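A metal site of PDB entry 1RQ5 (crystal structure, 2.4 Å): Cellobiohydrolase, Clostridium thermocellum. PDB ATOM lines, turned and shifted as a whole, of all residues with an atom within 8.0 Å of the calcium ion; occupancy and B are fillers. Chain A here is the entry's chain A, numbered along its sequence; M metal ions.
The backbone carbonyl oxygen of Gln 222 sits close to the side-chain carboxylate of Asp 214, 2.5 Å away. OD1 of Asp 214 lies within hydrogen-bond range of N of Gly 225 (3.0 Å). N of Gly 215 lies close to OD2 of Asp 228. N of Asp 228 lies within hydrogen-bond range of O of Arg 213. The side-chain carboxylate (OD2) of Asp 228 sits at hydrogen-bond distance from the backbone NH (N) of Gly 216, 3.2 Å away. OD2 of Asp 228 is in hydrogen-bond range of N of Met 217 (2.9 Å). The backbone carbonyl oxygen (O) of Gln 222 sits at hydrogen-bond distance from the backbone NH (N) of Gly 215, at 2.6 Å.
The calcium ion is bound by the side-chain carboxylate (OD1) of Asp 231, the side-chain carboxylate (OD2) of Asp 214, the backbone carbonyl oxygen (O) of Glu 221, the backbone carbonyl oxygen (O) of Tyr 226, the side-chain carboxylate (OD1) of Asp 228 and the side-chain amide oxygen (OD1) of Asn 224. The calcium ion has six donor atoms within binding distance.
Residues that only touch the calcium ion: Gln 222 (3.9 Å). Seven residues have an atom within 4 Å of the calcium ion: Asp 214, Glu 221, Gln 222, Asn 224, Tyr 226, Asp 228 and Asp 231. Along chain A the residues within 4 Å of the calcium ion span positions 214 to 231.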
ATOM      1  N   PRO A 211      11.792  -6.652  -2.726  1.00  0.00           N
ATOM      2  CA  PRO A 211      10.569  -7.420  -2.506  1.00  0.00           C
ATOM      3  C   PRO A 211       9.352  -6.626  -2.024  1.00  0.00           C
ATOM      4  O   PRO A 211       8.264  -7.172  -1.905  1.00  0.00           O
ATOM      5  CB  PRO A 211      11.000  -8.451  -1.484  1.00  0.00           C
ATOM      6  CG  PRO A 211      11.936  -7.654  -0.631  1.00  0.00           C
ATOM      7  CD  PRO A 211      12.772  -6.911  -1.654  1.00  0.00           C
ATOM      8  N   TYR A 212       9.544  -5.355  -1.740  1.00  0.00           N
ATOM      9  CA  TYR A 212       8.440  -4.534  -1.275  1.00  0.00           C
ATOM     10  C   TYR A 212       7.481  -4.097  -2.383  1.00  0.00           C
ATOM     11  O   TYR A 212       6.415  -3.551  -2.115  1.00  0.00           O
ATOM     12  CB  TYR A 212       9.001  -3.300  -0.582  1.00  0.00           C
ATOM     13  CG  TYR A 212       9.976  -3.639   0.532  1.00  0.00           C
ATOM     14  CD1 TYR A 212       9.531  -4.182   1.736  1.00  0.00           C
ATOM     15  CD2 TYR A 212      11.342  -3.401   0.370  1.00  0.00           C
ATOM     16  CE1 TYR A 212      10.420  -4.470   2.770  1.00  0.00           C
ATOM     17  CE2 TYR A 212      12.242  -3.690   1.395  1.00  0.00           C
ATOM     18  CZ  TYR A 212      11.778  -4.221   2.597  1.00  0.00           C
ATOM     19  OH  TYR A 212      12.656  -4.476   3.627  1.00  0.00           O
ATOM     20  N   ARG A 213       7.853  -4.346  -3.641  1.00  0.00           N
ATOM     21  CA  ARG A 213       7.013  -3.927  -4.744  1.00  0.00           C
ATOM     22  C   ARG A 213       6.326  -5.092  -5.441  1.00  0.00           C
ATOM     23  O   ARG A 213       6.752  -6.244  -5.300  1.00  0.00           O
ATOM     24  CB  ARG A 213       7.848  -3.171  -5.769  1.00  0.00           C
ATOM     25  CG  ARG A 213       8.881  -4.026  -6.468  1.00  0.00           C
ATOM     26  CD  ARG A 213       9.601  -3.260  -7.540  1.00  0.00           C
ATOM     27  NE  ARG A 213      10.082  -4.176  -8.579  1.00  0.00           N
ATOM     28  CZ  ARG A 213      11.013  -5.113  -8.389  1.00  0.00           C
ATOM     29  NH1 ARG A 213      11.581  -5.251  -7.199  1.00  0.00           N
ATOM     30  NH2 ARG A 213      11.379  -5.892  -9.398  1.00  0.00           N
ATOM     31  N   ASP A 214       5.261  -4.769  -6.181  1.00  0.00           N
ATOM     32  CA  ASP A 214       4.498  -5.745  -6.963  1.00  0.00           C
ATOM     33  C   ASP A 214       5.530  -6.267  -7.969  1.00  0.00           C
ATOM     34  O   ASP A 214       6.196  -5.473  -8.657  1.00  0.00           O
ATOM     35  CB  ASP A 214       3.323  -5.060  -7.689  1.00  0.00           C
ATOM     36  CG  ASP A 214       2.434  -6.054  -8.472  1.00  0.00           C
ATOM     37  OD1 ASP A 214       1.780  -5.623  -9.447  1.00  0.00           O
ATOM     38  OD2 ASP A 214       2.362  -7.249  -8.143  1.00  0.00           O
ATOM     39  N   GLY A 215       5.680  -7.577  -8.059  1.00  0.00           N
ATOM     40  CA  GLY A 215       6.661  -8.124  -8.979  1.00  0.00           C
ATOM     41  C   GLY A 215       8.056  -8.221  -8.385  1.00  0.00           C
ATOM     42  O   GLY A 215       9.024  -8.493  -9.088  1.00  0.00           O
ATOM     43  N   GLY A 216       8.158  -8.003  -7.076  1.00  0.00           N
ATOM     44  CA  GLY A 216       9.460  -8.080  -6.430  1.00  0.00           C
ATOM     45  C   GLY A 216       9.864  -9.467  -5.958  1.00  0.00           C
ATOM     46  O   GLY A 216      11.046  -9.712  -5.686  1.00  0.00           O
ATOM     47  N   MET A 217       8.891 -10.376  -5.870  1.00  0.00           N
ATOM     48  CA  MET A 217       9.139 -11.741  -5.429  1.00  0.00           C
ATOM     49  C   MET A 217       8.625 -12.749  -6.443  1.00  0.00           C
ATOM     50  O   MET A 217       7.600 -12.523  -7.091  1.00  0.00           O
ATOM     51  CB  MET A 217       8.459 -12.001  -4.090  1.00  0.00           C
ATOM     52  CG  MET A 217       9.056 -11.222  -2.945  1.00  0.00           C
ATOM     53  SD  MET A 217       7.863 -11.041  -1.634  1.00  0.00           S
ATOM     54  CE  MET A 217       7.862 -12.683  -0.936  1.00  0.00           C
ATOM     55  N   ILE A 219       6.711 -15.062  -6.686  1.00  0.00           N
ATOM     56  CA  ILE A 219       5.522 -15.719  -6.192  1.00  0.00           C
ATOM     57  C   ILE A 219       4.421 -15.543  -7.233  1.00  0.00           C
ATOM     58  O   ILE A 219       4.495 -14.658  -8.085  1.00  0.00           O
ATOM     59  CB  ILE A 219       5.085 -15.118  -4.859  1.00  0.00           C
ATOM     60  CG1 ILE A 219       4.805 -13.625  -5.044  1.00  0.00           C
ATOM     61  CG2 ILE A 219       6.195 -15.348  -3.806  1.00  0.00           C
ATOM     62  CD1 ILE A 219       4.306 -12.940  -3.785  1.00  0.00           C
ATOM     63  N   PRO A 220       3.368 -16.379  -7.161  1.00  0.00           N
ATOM     64  CA  PRO A 220       2.253 -16.293  -8.109  1.00  0.00           C
ATOM     65  C   PRO A 220       1.518 -14.957  -8.115  1.00  0.00           C
ATOM     66  O   PRO A 220       0.855 -14.632  -9.099  1.00  0.00           O
ATOM     67  CB  PRO A 220       1.336 -17.444  -7.670  1.00  0.00           C
ATOM     68  CG  PRO A 220       2.227 -18.363  -6.959  1.00  0.00           C
ATOM     69  CD  PRO A 220       3.118 -17.436  -6.182  1.00  0.00           C
ATOM     70  N   GLU A 221       1.622 -14.175  -7.036  1.00  0.00           N
ATOM     71  CA  GLU A 221       0.963 -12.860  -6.988  1.00  0.00           C
ATOM     72  C   GLU A 221       1.877 -11.786  -7.569  1.00  0.00           C
ATOM     73  O   GLU A 221       1.697 -10.616  -7.304  1.00  0.00           O
ATOM     74  CB  GLU A 221       0.591 -12.452  -5.549  1.00  0.00           C
ATOM     75  CG  GLU A 221      -0.415 -13.358  -4.850  1.00  0.00           C
ATOM     76  CD  GLU A 221       0.197 -14.677  -4.339  1.00  0.00           C
ATOM     77  OE1 GLU A 221       1.438 -14.775  -4.161  1.00  0.00           O
ATOM     78  OE2 GLU A 221      -0.571 -15.615  -4.085  1.00  0.00           O
ATOM     79  N   GLN A 222       2.856 -12.181  -8.370  1.00  0.00           N
ATOM     80  CA  GLN A 222       3.793 -11.253  -8.997  1.00  0.00           C
ATOM     81  C   GLN A 222       3.254  -9.939  -9.575  1.00  0.00           C
ATOM     82  O   GLN A 222       3.857  -8.896  -9.360  1.00  0.00           O
ATOM     83  CB  GLN A 222       4.553 -11.963 -10.110  1.00  0.00           C
ATOM     84  CG  GLN A 222       5.884 -12.483  -9.689  1.00  0.00           C
ATOM     85  CD  GLN A 222       6.520 -13.269 -10.799  1.00  0.00           C
ATOM     86  OE1 GLN A 222       5.888 -14.142 -11.376  1.00  0.00           O
ATOM     87  NE2 GLN A 222       7.770 -12.965 -11.116  1.00  0.00           N
ATOM     88  N   ASN A 223       2.186  -9.962 -10.353  1.00  0.00           N
ATOM     89  CA  ASN A 223       1.690  -8.696 -10.884  1.00  0.00           C
ATOM     90  C   ASN A 223       0.183  -8.587 -10.782  1.00  0.00           C
ATOM     91  O   ASN A 223      -0.525  -8.557 -11.777  1.00  0.00           O
ATOM     92  CB  ASN A 223       2.155  -8.484 -12.329  1.00  0.00           C
ATOM     93  CG  ASN A 223       3.616  -8.055 -12.420  1.00  0.00           C
ATOM     94  OD1 ASN A 223       4.500  -8.849 -12.791  1.00  0.00           O
ATOM     95  ND2 ASN A 223       3.886  -6.813 -12.055  1.00  0.00           N
ATOM     96  N   ASN A 224      -0.294  -8.518  -9.540  1.00  0.00           N
ATOM     97  CA  ASN A 224      -1.715  -8.423  -9.265  1.00  0.00           C
ATOM     98  C   ASN A 224      -2.043  -7.065  -8.663  1.00  0.00           C
ATOM     99  O   ASN A 224      -3.096  -6.888  -8.033  1.00  0.00           O
ATOM    100  CB  ASN A 224      -2.119  -9.564  -8.334  1.00  0.00           C
ATOM    101  CG  ASN A 224      -1.690  -9.347  -6.884  1.00  0.00           C
ATOM    102  OD1 ASN A 224      -0.884  -8.479  -6.569  1.00  0.00           O
ATOM    103  ND2 ASN A 224      -2.252 -10.148  -6.000  1.00  0.00           N
ATOM    104  N   GLY A 225      -1.133  -6.120  -8.845  1.00  0.00           N
ATOM    105  CA  GLY A 225      -1.319  -4.774  -8.349  1.00  0.00           C
ATOM    106  C   GLY A 225      -0.929  -4.477  -6.908  1.00  0.00           C
ATOM    107  O   GLY A 225      -0.842  -3.310  -6.534  1.00  0.00           O
ATOM    108  N   TYR A 226      -0.667  -5.509  -6.109  1.00  0.00           N
ATOM    109  CA  TYR A 226      -0.317  -5.321  -4.705  1.00  0.00           C
ATOM    110  C   TYR A 226       1.158  -5.517  -4.400  1.00  0.00           C
ATOM    111  O   TYR A 226       1.888  -6.097  -5.181  1.00  0.00           O
ATOM    112  CB  TYR A 226      -1.122  -6.276  -3.830  1.00  0.00           C
ATOM    113  CG  TYR A 226      -2.598  -6.229  -4.084  1.00  0.00           C
ATOM    114  CD1 TYR A 226      -3.230  -5.035  -4.394  1.00  0.00           C
ATOM    115  CD2 TYR A 226      -3.378  -7.387  -3.955  1.00  0.00           C
ATOM    116  CE1 TYR A 226      -4.612  -4.972  -4.569  1.00  0.00           C
ATOM    117  CE2 TYR A 226      -4.765  -7.331  -4.125  1.00  0.00           C
ATOM    118  CZ  TYR A 226      -5.365  -6.109  -4.429  1.00  0.00           C
ATOM    119  OH  TYR A 226      -6.729  -6.009  -4.617  1.00  0.00           O
ATOM    120  N   PRO A 227       1.637  -5.001  -3.272  1.00  0.00           N
ATOM    121  CA  PRO A 227       3.061  -5.209  -2.988  1.00  0.00           C
ATOM    122  C   PRO A 227       3.305  -6.695  -2.687  1.00  0.00           C
ATOM    123  O   PRO A 227       2.600  -7.275  -1.872  1.00  0.00           O
ATOM    124  CB  PRO A 227       3.316  -4.290  -1.785  1.00  0.00           C
ATOM    125  CG  PRO A 227       2.297  -3.182  -2.004  1.00  0.00           C
ATOM    126  CD  PRO A 227       1.068  -3.936  -2.425  1.00  0.00           C
ATOM    127  N   ASP A 228       4.296  -7.304  -3.345  1.00  0.00           N
ATOM    128  CA  ASP A 228       4.557  -8.732  -3.154  1.00  0.00           C
ATOM    129  C   ASP A 228       4.749  -9.204  -1.720  1.00  0.00           C
ATOM    130  O   ASP A 228       4.149 -10.210  -1.324  1.00  0.00           O
ATOM    131  CB  ASP A 228       5.751  -9.180  -3.997  1.00  0.00           C
ATOM    132  CG  ASP A 228       5.399  -9.374  -5.462  1.00  0.00           C
ATOM    133  OD1 ASP A 228       4.471  -8.708  -5.941  1.00  0.00           O
ATOM    134  OD2 ASP A 228       6.039 -10.169  -6.167  1.00  0.00           O
ATOM    135  N   ILE A 229       5.575  -8.527  -0.938  1.00  0.00           N
ATOM    136  CA  ILE A 229       5.748  -8.965   0.434  1.00  0.00           C
ATOM    137  C   ILE A 229       4.385  -8.997   1.177  1.00  0.00           C
ATOM    138  O   ILE A 229       4.161  -9.852   2.029  1.00  0.00           O
ATOM    139  CB  ILE A 229       6.750  -8.079   1.219  1.00  0.00           C
ATOM    140  CG1 ILE A 229       7.215  -8.835   2.461  1.00  0.00           C
ATOM    141  CG2 ILE A 229       6.080  -6.755   1.663  1.00  0.00           C
ATOM    142  CD1 ILE A 229       8.245  -8.096   3.288  1.00  0.00           C
ATOM    143  N   LEU A 230       3.463  -8.088   0.860  1.00  0.00           N
ATOM    144  CA  LEU A 230       2.163  -8.138   1.547  1.00  0.00           C
ATOM    145  C   LEU A 230       1.278  -9.285   1.022  1.00  0.00           C
ATOM    146  O   LEU A 230       0.386  -9.770   1.726  1.00  0.00           O
ATOM    147  CB  LEU A 230       1.415  -6.794   1.419  1.00  0.00           C
ATOM    148  CG  LEU A 230       1.962  -5.565   2.163  1.00  0.00           C
ATOM    149  CD1 LEU A 230       1.019  -4.377   1.923  1.00  0.00           C
ATOM    150  CD2 LEU A 230       2.088  -5.865   3.655  1.00  0.00           C
ATOM    151  N   ASP A 231       1.499  -9.712  -0.217  1.00  0.00           N
ATOM    152  CA  ASP A 231       0.700 -10.804  -0.748  1.00  0.00           C
ATOM    153  C   ASP A 231       0.982 -12.060   0.086  1.00  0.00           C
ATOM    154  O   ASP A 231       0.072 -12.827   0.403  1.00  0.00           O
ATOM    155  CB  ASP A 231       1.048 -11.048  -2.225  1.00  0.00           C
ATOM    156  CG  ASP A 231       0.373 -10.039  -3.157  1.00  0.00           C
ATOM    157  OD1 ASP A 231       1.057  -9.390  -3.979  1.00  0.00           O
ATOM    158  OD2 ASP A 231      -0.854  -9.892  -3.062  1.00  0.00           O
ATOM    159  N   GLU A 232       2.248 -12.235   0.453  1.00  0.00           N
ATOM    160  CA  GLU A 232       2.675 -13.368   1.251  1.00  0.00           C
ATOM    161  C   GLU A 232       2.048 -13.261   2.622  1.00  0.00           C
ATOM    162  O   GLU A 232       1.430 -14.186   3.096  1.00  0.00           O
ATOM    163  CB  GLU A 232       4.197 -13.393   1.411  1.00  0.00           C
ATOM    164  CG  GLU A 232       4.766 -14.702   1.899  1.00  0.00           C
ATOM    165  CD  GLU A 232       4.450 -15.854   0.965  1.00  0.00           C
ATOM    166  OE1 GLU A 232       4.981 -15.855  -0.173  1.00  0.00           O
ATOM    167  OE2 GLU A 232       3.654 -16.746   1.368  1.00  0.00           O
ATOM    168  N   TRP A 304      -2.768  -2.360   3.976  1.00  0.00           N
ATOM    169  CA  TRP A 304      -3.506  -2.705   2.768  1.00  0.00           C
ATOM    170  C   TRP A 304      -4.579  -1.705   2.365  1.00  0.00           C
ATOM    171  O   TRP A 304      -5.206  -1.855   1.331  1.00  0.00           O
ATOM    172  CB  TRP A 304      -4.201  -4.064   2.925  1.00  0.00           C
ATOM    173  CG  TRP A 304      -3.349  -5.257   2.622  1.00  0.00           C
ATOM    174  CD1 TRP A 304      -2.597  -5.984   3.492  1.00  0.00           C
ATOM    175  CD2 TRP A 304      -3.215  -5.881   1.347  1.00  0.00           C
ATOM    176  NE1 TRP A 304      -1.992  -7.029   2.833  1.00  0.00           N
ATOM    177  CE2 TRP A 304      -2.355  -6.993   1.520  1.00  0.00           C
ATOM    178  CE3 TRP A 304      -3.723  -5.609   0.066  1.00  0.00           C
ATOM    179  CZ2 TRP A 304      -2.006  -7.848   0.445  1.00  0.00           C
ATOM    180  CZ3 TRP A 304      -3.375  -6.445  -0.988  1.00  0.00           C
ATOM    181  CH2 TRP A 304      -2.522  -7.545  -0.788  1.00  0.00           C
HETATM  182 CA    CA M   1       1.834  -8.467  -6.061  1.00  0.00          CA
